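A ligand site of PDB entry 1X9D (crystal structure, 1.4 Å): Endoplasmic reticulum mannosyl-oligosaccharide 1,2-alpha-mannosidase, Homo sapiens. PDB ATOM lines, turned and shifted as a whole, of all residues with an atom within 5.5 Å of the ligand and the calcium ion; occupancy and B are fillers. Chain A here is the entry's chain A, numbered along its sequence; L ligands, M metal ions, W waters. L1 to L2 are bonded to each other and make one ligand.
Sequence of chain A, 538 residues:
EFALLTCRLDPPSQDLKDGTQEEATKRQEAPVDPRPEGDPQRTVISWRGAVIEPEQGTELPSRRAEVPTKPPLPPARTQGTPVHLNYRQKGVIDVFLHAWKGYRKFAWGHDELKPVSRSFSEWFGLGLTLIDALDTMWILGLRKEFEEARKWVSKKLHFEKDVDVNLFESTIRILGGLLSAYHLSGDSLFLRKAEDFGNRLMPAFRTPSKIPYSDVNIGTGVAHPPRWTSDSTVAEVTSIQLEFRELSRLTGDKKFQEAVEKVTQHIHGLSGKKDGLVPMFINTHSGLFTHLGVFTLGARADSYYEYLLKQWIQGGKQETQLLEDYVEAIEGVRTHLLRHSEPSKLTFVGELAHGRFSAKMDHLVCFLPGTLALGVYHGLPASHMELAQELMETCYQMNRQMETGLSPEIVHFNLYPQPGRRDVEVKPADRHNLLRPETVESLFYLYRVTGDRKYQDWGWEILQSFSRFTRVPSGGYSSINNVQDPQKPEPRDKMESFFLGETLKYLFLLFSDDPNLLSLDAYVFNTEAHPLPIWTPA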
ATOM      1  N   PHE A 168      -2.166  12.240 -10.680  1.00  0.00           N
ATOM      2  CA  PHE A 168      -1.513  11.006 -11.062  1.00  0.00           C
ATOM      3  C   PHE A 168      -2.415   9.778 -10.883  1.00  0.00           C
ATOM      4  O   PHE A 168      -2.553   8.958 -11.792  1.00  0.00           O
ATOM      5  CB  PHE A 168      -0.181  10.882 -10.288  1.00  0.00           C
ATOM      6  CG  PHE A 168       0.349   9.494 -10.154  1.00  0.00           C
ATOM      7  CD1 PHE A 168       0.184   8.804  -8.959  1.00  0.00           C
ATOM      8  CD2 PHE A 168       1.073   8.883 -11.169  1.00  0.00           C
ATOM      9  CE1 PHE A 168       0.716   7.507  -8.801  1.00  0.00           C
ATOM     10  CE2 PHE A 168       1.602   7.585 -10.987  1.00  0.00           C
ATOM     11  CZ  PHE A 168       1.411   6.921  -9.785  1.00  0.00           C
ATOM     12  N   GLU A 169      -3.030   9.627  -9.732  1.00  0.00           N
ATOM     13  CA  GLU A 169      -3.841   8.426  -9.497  1.00  0.00           C
ATOM     14  C   GLU A 169      -5.018   8.383 -10.459  1.00  0.00           C
ATOM     15  O   GLU A 169      -5.372   7.328 -10.969  1.00  0.00           O
ATOM     16  CB  GLU A 169      -4.356   8.402  -8.059  1.00  0.00           C
ATOM     17  CG  GLU A 169      -3.296   8.255  -7.005  1.00  0.00           C
ATOM     18  CD  GLU A 169      -2.743   6.856  -6.919  1.00  0.00           C
ATOM     19  OE1 GLU A 169      -3.247   5.979  -7.634  1.00  0.00           O
ATOM     20  OE2 GLU A 169      -1.822   6.636  -6.153  1.00  0.00           O
ATOM     21  N   ILE A 172      -3.574   7.460 -14.124  1.00  0.00           N
ATOM     22  CA  ILE A 172      -3.140   6.071 -14.407  1.00  0.00           C
ATOM     23  C   ILE A 172      -4.290   5.074 -14.314  1.00  0.00           C
ATOM     24  O   ILE A 172      -4.317   4.102 -15.062  1.00  0.00           O
ATOM     25  CB  ILE A 172      -1.956   5.669 -13.523  1.00  0.00           C
ATOM     26  CG1 ILE A 172      -2.356   5.525 -12.038  1.00  0.00           C
ATOM     27  CG2 ILE A 172      -0.797   6.650 -13.744  1.00  0.00           C
ATOM     28  CD1 ILE A 172      -1.242   4.998 -11.162  1.00  0.00           C
ATOM     29  N   ARG A 173      -5.251   5.330 -13.436  1.00  0.00           N
ATOM     30  CA  ARG A 173      -6.367   4.402 -13.212  1.00  0.00           C
ATOM     31  C   ARG A 173      -7.533   4.708 -14.156  1.00  0.00           C
ATOM     32  O   ARG A 173      -7.966   3.854 -14.953  1.00  0.00           O
ATOM     33  CB  ARG A 173      -6.807   4.419 -11.745  1.00  0.00           C
ATOM     34  CG  ARG A 173      -5.671   4.110 -10.747  1.00  0.00           C
ATOM     35  CD  ARG A 173      -6.139   3.705  -9.254  1.00  0.00           C
ATOM     36  NE  ARG A 173      -5.044   3.797  -8.265  1.00  0.00           N
ATOM     37  CZ  ARG A 173      -5.041   3.178  -7.115  1.00  0.00           C
ATOM     38  NH1 ARG A 173      -6.061   2.375  -6.783  1.00  0.00           N
ATOM     39  NH2 ARG A 173      -4.057   3.366  -6.306  1.00  0.00           N
ATOM     40  N   THR A 233       5.202  15.559  -6.478  1.00  0.00           N
ATOM     41  CA  THR A 233       5.983  14.350  -6.427  1.00  0.00           C
ATOM     42  C   THR A 233       6.503  14.032  -7.828  1.00  0.00           C
ATOM     43  O   THR A 233       5.742  14.037  -8.797  1.00  0.00           O
ATOM     44  CB  THR A 233       5.084  13.210  -5.891  1.00  0.00           C
ATOM     45  OG1 THR A 233       4.715  13.491  -4.520  1.00  0.00           O
ATOM     46  CG2 THR A 233       5.802  11.903  -5.838  1.00  0.00           C
ATOM     47  N   ALA A 235       7.574  11.268  -9.454  1.00  0.00           N
ATOM     48  CA  ALA A 235       6.932  10.189 -10.203  1.00  0.00           C
ATOM     49  C   ALA A 235       5.550  10.589 -10.647  1.00  0.00           C
ATOM     50  O   ALA A 235       5.110  10.198 -11.722  1.00  0.00           O
ATOM     51  CB  ALA A 235       6.844   8.914  -9.372  1.00  0.00           C
ATOM     52  N   GLU A 236       4.829  11.364  -9.839  1.00  0.00           N
ATOM     53  CA  GLU A 236       3.465  11.727 -10.204  1.00  0.00           C
ATOM     54  C   GLU A 236       3.398  12.606 -11.437  1.00  0.00           C
ATOM     55  O   GLU A 236       2.488  12.438 -12.246  1.00  0.00           O
ATOM     56  CB  GLU A 236       2.730  12.389  -9.008  1.00  0.00           C
ATOM     57  CG  GLU A 236       2.494  11.398  -7.906  1.00  0.00           C
ATOM     58  CD  GLU A 236       1.578  11.877  -6.792  1.00  0.00           C
ATOM     59  OE1 GLU A 236       0.973  12.974  -6.887  1.00  0.00           O
ATOM     60  OE2 GLU A 236       1.445  11.125  -5.801  1.00  0.00           O
ATOM     61  N   GLY A 298      12.015   3.593  -5.333  1.00  0.00           N
ATOM     62  CA  GLY A 298      10.703   3.196  -4.854  1.00  0.00           C
ATOM     63  C   GLY A 298       9.715   4.339  -4.933  1.00  0.00           C
ATOM     64  O   GLY A 298       9.743   5.159  -5.862  1.00  0.00           O
ATOM     65  N   ALA A 299       8.836   4.421  -3.934  1.00  0.00           N
ATOM     66  CA  ALA A 299       7.747   5.363  -3.961  1.00  0.00           C
ATOM     67  C   ALA A 299       8.295   6.755  -4.166  1.00  0.00           C
ATOM     68  O   ALA A 299       9.283   7.149  -3.545  1.00  0.00           O
ATOM     69  CB  ALA A 299       6.946   5.299  -2.657  1.00  0.00           C
ATOM     70  N   ARG A 300       7.616   7.496  -5.067  1.00  0.00           N
ATOM     71  CA  ARG A 300       7.859   8.918  -5.429  1.00  0.00           C
ATOM     72  C   ARG A 300       8.803   9.103  -6.583  1.00  0.00           C
ATOM     73  O   ARG A 300       8.908  10.193  -7.111  1.00  0.00           O
ATOM     74  CB  ARG A 300       8.311   9.769  -4.257  1.00  0.00           C
ATOM     75  CG  ARG A 300       7.327   9.838  -3.138  1.00  0.00           C
ATOM     76  CD  ARG A 300       7.651  10.925  -2.133  1.00  0.00           C
ATOM     77  NE  ARG A 300       6.778  10.875  -0.983  1.00  0.00           N
ATOM     78  N   ALA A 301       9.516   8.037  -6.989  1.00  0.00           N
ATOM     79  CA  ALA A 301      10.422   8.126  -8.146  1.00  0.00           C
ATOM     80  C   ALA A 301      10.286   6.970  -9.167  1.00  0.00           C
ATOM     81  O   ALA A 301      10.401   7.216 -10.345  1.00  0.00           O
ATOM     82  CB  ALA A 301      11.871   8.227  -7.658  1.00  0.00           C
ATOM     83  N   ASP A 302      10.082   5.739  -8.699  1.00  0.00           N
ATOM     84  CA  ASP A 302       9.931   4.547  -9.551  1.00  0.00           C
ATOM     85  C   ASP A 302       9.457   4.768 -10.978  1.00  0.00           C
ATOM     86  O   ASP A 302      10.182   4.488 -11.918  1.00  0.00           O
ATOM     87  CB  ASP A 302       9.051   3.468  -8.858  1.00  0.00           C
ATOM     88  CG  ASP A 302       7.770   3.971  -8.286  1.00  0.00           C
ATOM     89  OD1 ASP A 302       7.307   5.105  -8.534  1.00  0.00           O
ATOM     90  OD2 ASP A 302       7.122   3.171  -7.563  1.00  0.00           O
ATOM     91  N   SER A 303       8.219   5.214 -11.160  1.00  0.00           N
ATOM     92  CA  SER A 303       7.626   5.180 -12.478  1.00  0.00           C
ATOM     93  C   SER A 303       8.137   6.280 -13.396  1.00  0.00           C
ATOM     94  O   SER A 303       7.902   6.214 -14.605  1.00  0.00           O
ATOM     95  CB  SER A 303       6.085   5.110 -12.390  1.00  0.00           C
ATOM     96  OG  SER A 303       5.548   6.118 -11.558  1.00  0.00           O
ATOM     97  N   GLU A 306      10.358   4.084 -15.477  1.00  0.00           N
ATOM     98  CA  GLU A 306       9.475   3.272 -16.289  1.00  0.00           C
ATOM     99  C   GLU A 306       8.948   4.027 -17.482  1.00  0.00           C
ATOM    100  O   GLU A 306       8.940   3.516 -18.592  1.00  0.00           O
ATOM    101  CB  GLU A 306       8.300   2.808 -15.392  1.00  0.00           C
ATOM    102  CG  GLU A 306       7.278   1.880 -16.017  1.00  0.00           C
ATOM    103  CD  GLU A 306       6.036   1.709 -15.148  1.00  0.00           C
ATOM    104  OE1 GLU A 306       5.089   1.038 -15.616  1.00  0.00           O
ATOM    105  OE2 GLU A 306       6.005   2.224 -14.005  1.00  0.00           O
ATOM    106  N   LEU A 364       7.592  -1.792  -4.323  1.00  0.00           N
ATOM    107  CA  LEU A 364       7.428  -1.013  -5.556  1.00  0.00           C
ATOM    108  C   LEU A 364       8.610  -1.115  -6.492  1.00  0.00           C
ATOM    109  O   LEU A 364       8.442  -1.047  -7.722  1.00  0.00           O
ATOM    110  CB  LEU A 364       7.176   0.425  -5.216  1.00  0.00           C
ATOM    111  CG  LEU A 364       5.807   0.713  -4.583  1.00  0.00           C
ATOM    112  CD1 LEU A 364       5.799   2.074  -3.893  1.00  0.00           C
ATOM    113  CD2 LEU A 364       4.677   0.598  -5.606  1.00  0.00           C
ATOM    114  N   ARG A 436      -0.319  -6.028  -4.104  1.00  0.00           N
ATOM    115  CA  ARG A 436       0.361  -5.252  -5.109  1.00  0.00           C
ATOM    116  C   ARG A 436       0.886  -6.153  -6.233  1.00  0.00           C
ATOM    117  O   ARG A 436       1.242  -7.296  -6.013  1.00  0.00           O
ATOM    118  CB  ARG A 436       1.543  -4.473  -4.518  1.00  0.00           C
ATOM    119  CG  ARG A 436       1.162  -3.276  -3.650  1.00  0.00           C
ATOM    120  CD  ARG A 436       2.371  -2.363  -3.409  1.00  0.00           C
ATOM    121  NE  ARG A 436       2.135  -1.299  -2.441  1.00  0.00           N
ATOM    122  CZ  ARG A 436       1.502  -0.149  -2.689  1.00  0.00           C
ATOM    123  NH1 ARG A 436       1.017   0.134  -3.893  1.00  0.00           N
ATOM    124  NH2 ARG A 436       1.382   0.746  -1.704  1.00  0.00           N
ATOM    125  N   PRO A 437       0.934  -5.600  -7.438  1.00  0.00           N
ATOM    126  CA  PRO A 437       1.288  -6.356  -8.656  1.00  0.00           C
ATOM    127  C   PRO A 437       2.737  -6.460  -9.068  1.00  0.00           C
ATOM    128  O   PRO A 437       2.996  -7.182 -10.020  1.00  0.00           O
ATOM    129  CB  PRO A 437       0.565  -5.570  -9.725  1.00  0.00           C
ATOM    130  CG  PRO A 437       0.705  -4.169  -9.260  1.00  0.00           C
ATOM    131  CD  PRO A 437       0.439  -4.230  -7.782  1.00  0.00           C
ATOM    132  N   GLU A 438       3.671  -5.766  -8.436  1.00  0.00           N
ATOM    133  CA  GLU A 438       4.957  -5.520  -9.113  1.00  0.00           C
ATOM    134  C   GLU A 438       5.769  -6.775  -9.332  1.00  0.00           C
ATOM    135  O   GLU A 438       6.481  -6.862 -10.344  1.00  0.00           O
ATOM    136  CB  GLU A 438       5.797  -4.460  -8.407  1.00  0.00           C
ATOM    137  CG  GLU A 438       5.203  -3.057  -8.501  1.00  0.00           C
ATOM    138  CD  GLU A 438       4.066  -2.825  -7.539  1.00  0.00           C
ATOM    139  OE1 GLU A 438       3.326  -1.848  -7.751  1.00  0.00           O
ATOM    140  OE2 GLU A 438       3.910  -3.606  -6.584  1.00  0.00           O
ATOM    141  N   GLU A 441       3.933  -8.560 -12.284  1.00  0.00           N
ATOM    142  CA  GLU A 441       4.198  -7.713 -13.443  1.00  0.00           C
ATOM    143  C   GLU A 441       5.560  -8.073 -14.063  1.00  0.00           C
ATOM    144  O   GLU A 441       5.675  -8.324 -15.252  1.00  0.00           O
ATOM    145  CB  GLU A 441       4.167  -6.240 -13.001  1.00  0.00           C
ATOM    146  CG  GLU A 441       4.587  -5.236 -14.035  1.00  0.00           C
ATOM    147  CD  GLU A 441       4.642  -3.815 -13.495  1.00  0.00           C
ATOM    148  OE1 GLU A 441       4.992  -2.903 -14.282  1.00  0.00           O
ATOM    149  OE2 GLU A 441       4.320  -3.637 -12.322  1.00  0.00           O
ATOM    150  N   PHE A 498      -6.049  -2.028  -7.994  1.00  0.00           N
ATOM    151  CA  PHE A 498      -4.962  -2.633  -8.758  1.00  0.00           C
ATOM    152  C   PHE A 498      -4.840  -4.133  -8.592  1.00  0.00           C
ATOM    153  O   PHE A 498      -4.129  -4.760  -9.367  1.00  0.00           O
ATOM    154  CB  PHE A 498      -3.624  -1.909  -8.503  1.00  0.00           C
ATOM    155  CG  PHE A 498      -3.250  -1.720  -7.040  1.00  0.00           C
ATOM    156  CD1 PHE A 498      -2.871  -2.793  -6.249  1.00  0.00           C
ATOM    157  CD2 PHE A 498      -3.198  -0.435  -6.478  1.00  0.00           C
ATOM    158  CE1 PHE A 498      -2.488  -2.613  -4.925  1.00  0.00           C
ATOM    159  CE2 PHE A 498      -2.819  -0.254  -5.172  1.00  0.00           C
ATOM    160  CZ  PHE A 498      -2.460  -1.336  -4.411  1.00  0.00           C
ATOM    161  N   GLU A 502      -4.375  -4.882 -12.161  1.00  0.00           N
ATOM    162  CA  GLU A 502      -3.017  -5.246 -12.465  1.00  0.00           C
ATOM    163  C   GLU A 502      -2.650  -6.669 -12.078  1.00  0.00           C
ATOM    164  O   GLU A 502      -2.200  -7.436 -12.922  1.00  0.00           O
ATOM    165  CB  GLU A 502      -2.031  -4.308 -11.777  1.00  0.00           C
ATOM    166  CG  GLU A 502      -2.178  -2.849 -12.061  1.00  0.00           C
ATOM    167  CD  GLU A 502      -0.918  -2.079 -11.656  1.00  0.00           C
ATOM    168  OE1 GLU A 502      -1.031  -1.201 -10.774  1.00  0.00           O
ATOM    169  OE2 GLU A 502       0.193  -2.384 -12.197  1.00  0.00           O
ATOM    170  N   THR A 527       1.342   2.343 -16.165  1.00  0.00           N
ATOM    171  CA  THR A 527       1.841   1.887 -14.860  1.00  0.00           C
ATOM    172  C   THR A 527       0.749   1.274 -13.985  1.00  0.00           C
ATOM    173  O   THR A 527       1.037   0.808 -12.890  1.00  0.00           O
ATOM    174  CB  THR A 527       2.625   3.000 -14.156  1.00  0.00           C
ATOM    175  OG1 THR A 527       3.458   2.430 -13.130  1.00  0.00           O
ATOM    176  CG2 THR A 527       1.687   4.032 -13.524  1.00  0.00           C
ATOM    177  N   GLU A 528      -0.497   1.261 -14.473  1.00  0.00           N
ATOM    178  CA  GLU A 528      -1.618   0.540 -13.860  1.00  0.00           C
ATOM    179  C   GLU A 528      -2.104  -0.569 -14.796  1.00  0.00           C
ATOM    180  O   GLU A 528      -3.298  -0.942 -14.796  1.00  0.00           O
ATOM    181  CB  GLU A 528      -2.751   1.516 -13.484  1.00  0.00           C
ATOM    182  CG  GLU A 528      -3.810   0.925 -12.551  1.00  0.00           C
ATOM    183  CD  GLU A 528      -3.662   1.245 -11.086  1.00  0.00           C
ATOM    184  OE1 GLU A 528      -2.700   1.898 -10.687  1.00  0.00           O
ATOM    185  OE2 GLU A 528      -4.555   0.821 -10.298  1.00  0.00           O
HETATM  186  S1  LIG L   1       1.663   4.046  -7.173  1.00  0.00           S
HETATM  187  C1  LIG L   1       2.919   4.105  -5.861  1.00  0.00           C
HETATM  188  C2  LIG L   1       2.471   4.998  -4.737  1.00  0.00           C
HETATM  189  O1  LIG L   1       3.392   4.804  -3.661  1.00  0.00           O
HETATM  190  C3  LIG L   1       2.972   5.390  -2.411  1.00  0.00           C
HETATM  191  O2  LIG L   1       2.429   6.350  -5.167  1.00  0.00           O
HETATM  192  C4  LIG L   1       4.296   4.580  -6.355  1.00  0.00           C
HETATM  193  O3  LIG L   1       4.689   3.774  -7.452  1.00  0.00           O
HETATM  194  C5  LIG L   1       4.288   6.081  -6.714  1.00  0.00           C
HETATM  195  O4  LIG L   1       5.652   6.538  -6.902  1.00  0.00           O
HETATM  196  C6  LIG L   1       3.689   6.906  -5.608  1.00  0.00           C
HETATM  197  C7  LIG L   1       3.420   8.299  -6.125  1.00  0.00           C
HETATM  198  O5  LIG L   1       3.111   9.162  -5.030  1.00  0.00           O
HETATM  199  C1  LG2 L   2       1.978   2.512  -8.106  1.00  0.00           C
HETATM  200  C2  LG2 L   2       1.282   2.619  -9.433  1.00  0.00           C
HETATM  201  C3  LG2 L   2       0.326   1.501  -9.715  1.00  0.00           C
HETATM  202  C4  LG2 L   2      -0.553   1.186  -8.531  1.00  0.00           C
HETATM  203  C5  LG2 L   2       0.321   0.785  -7.346  1.00  0.00           C
HETATM  204  C6  LG2 L   2       0.423  -0.741  -7.307  1.00  0.00           C
HETATM  205  O1  LG2 L   2       2.255   2.653 -10.471  1.00  0.00           O
HETATM  206  O2  LG2 L   2       1.051   0.286 -10.072  1.00  0.00           O
HETATM  207  O3  LG2 L   2      -1.429   2.307  -8.275  1.00  0.00           O
HETATM  208  O4  LG2 L   2       1.677   1.266  -7.419  1.00  0.00           O
HETATM  209  O5  LG2 L   2       1.285  -1.173  -6.267  1.00  0.00           O
HETATM  210 CA    CA M   1       3.059   0.608 -11.523  1.00  0.00          CA
HETATM  211  O   HOH W   1       3.702   9.329  -2.331  1.00  0.00           O
HETATM  212  O   HOH W   2       3.936  -0.503 -13.639  1.00  0.00           O
HETATM  213  O   HOH W   3       4.000   0.264  -9.302  1.00  0.00           O
HETATM  214  O   HOH W   4       3.909   4.635  -9.932  1.00  0.00           O
HETATM  215  O   HOH W   5       2.702  -1.730 -11.234  1.00  0.00           O
HETATM  216  O   HOH W   6       5.487   1.150 -11.481  1.00  0.00           O
HETATM  217  O   HOH W   7      -1.407   4.030  -6.191  1.00  0.00           O
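An oxygen (O2) of LG2 L2 sits close to the side-chain carboxylate of Glu 502 (2.7 Å). The guanidinium group of Arg 436 is in hydrogen-bond range of an oxygen (O5) of LG2 L2 (2.7 Å). An oxygen (O3) of LG2 L2 is in hydrogen-bond range of the side-chain carboxylate (OE1) of Glu 528 (2.8 Å). OD2 of Asp 302 sits at hydrogen-bond distance from O3 of LIG L1, at 2.5 Å. An oxygen (O5) of LIG L1 lies within hydrogen-bond range of the side-chain carboxylate (OE2) of Glu 236, 2.7 Å away. An oxygen (O4) of LIG L1 sits at hydrogen-bond distance from the backbone NH (N) of Arg 300. An oxygen (O5) of LG2 L2 is in hydrogen-bond range of the side-chain carboxylate (OE1) of Glu 438. The guanidinium group (NH2) of Arg 173 sits at hydrogen-bond distance from an oxygen (O3) of LG2 L2 (3.5 Å).
The guanidinium group (NE) of Arg 173 is in salt-bridge range of the side-chain carboxylate (OE1) of Glu 169 (2.9 Å). The side-chain hydroxyl (OG1) of Thr 527 lies close to the side-chain carboxylate (OE2) of Glu 306. N of Ala 235 is in hydrogen-bond range of O of Arg 300 (2.9 Å). OE2 of Glu 528 lies within salt-bridge range of NE of Arg 173 (3.6 Å).
Phe 168 touches the ligand. Ile 172 touches the ligand. Thr 233 touches the ligand. CB of Ala 235 touches O4 of LIG L1, 3.6 Å away. CB of Ala 299 touches O1 of LIG L1, at 3.7 Å. CD2 of Leu 364 touches O4 of LG2 L2, 3.6 Å away. CD of Pro 437 touches O5 of LG2 L2, 3.5 Å away. CD2 of Phe 498 touches C4 of LG2 L2 (3.7 Å). Hydrophobic or aromatic side chains that line the ligand: Phe 168, Ile 172, Ala 235, Ala 299, Leu 364, Pro 437 and Phe 498. Of the 23 residues printed, 17 come within 4 Å of the ligand.
Water W5 is bound to the calcium ion (2.4 Å). The calcium ion is bound by O1 of LG2 L2 (2.4 Å). Water W3 binds the calcium ion (2.4 Å). The calcium ion is bound by the backbone carbonyl oxygen (O) of Thr 527, at 2.4 Å. OG1 of Thr 527 is bound to the calcium ion. The calcium ion is bound by water W6 (2.5 Å). O2 of LG2 L2 binds the calcium ion (2.5 Å). The calcium ion is bound by water W2 (2.5 Å). The calcium ion has eight donor atoms within binding distance.
Water W3 lies within hydrogen-bond range of OE1 of Glu 438 and O4 of LG2 L2. Water W2 bridges OE1 of Glu 441 (2.7 Å) and OE1 of Glu 306 (2.8 Å). Water W5 bridges the side-chain carboxylate (OE2) of Glu 441 (2.7 Å) and the side-chain carboxylate (OE2) of Glu 502 (2.8 Å). Water W4 lies within hydrogen-bond range of O3 of LIG L1 (2.7 Å) and OG of Ser 303 (2.7 Å). Water W7 lies within hydrogen-bond range of the side-chain carboxylate of Glu 169 (2.6 Å), an oxygen (O3) of LG2 L2 (2.7 Å) and the guanidinium group of Arg 173 (2.7 Å).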
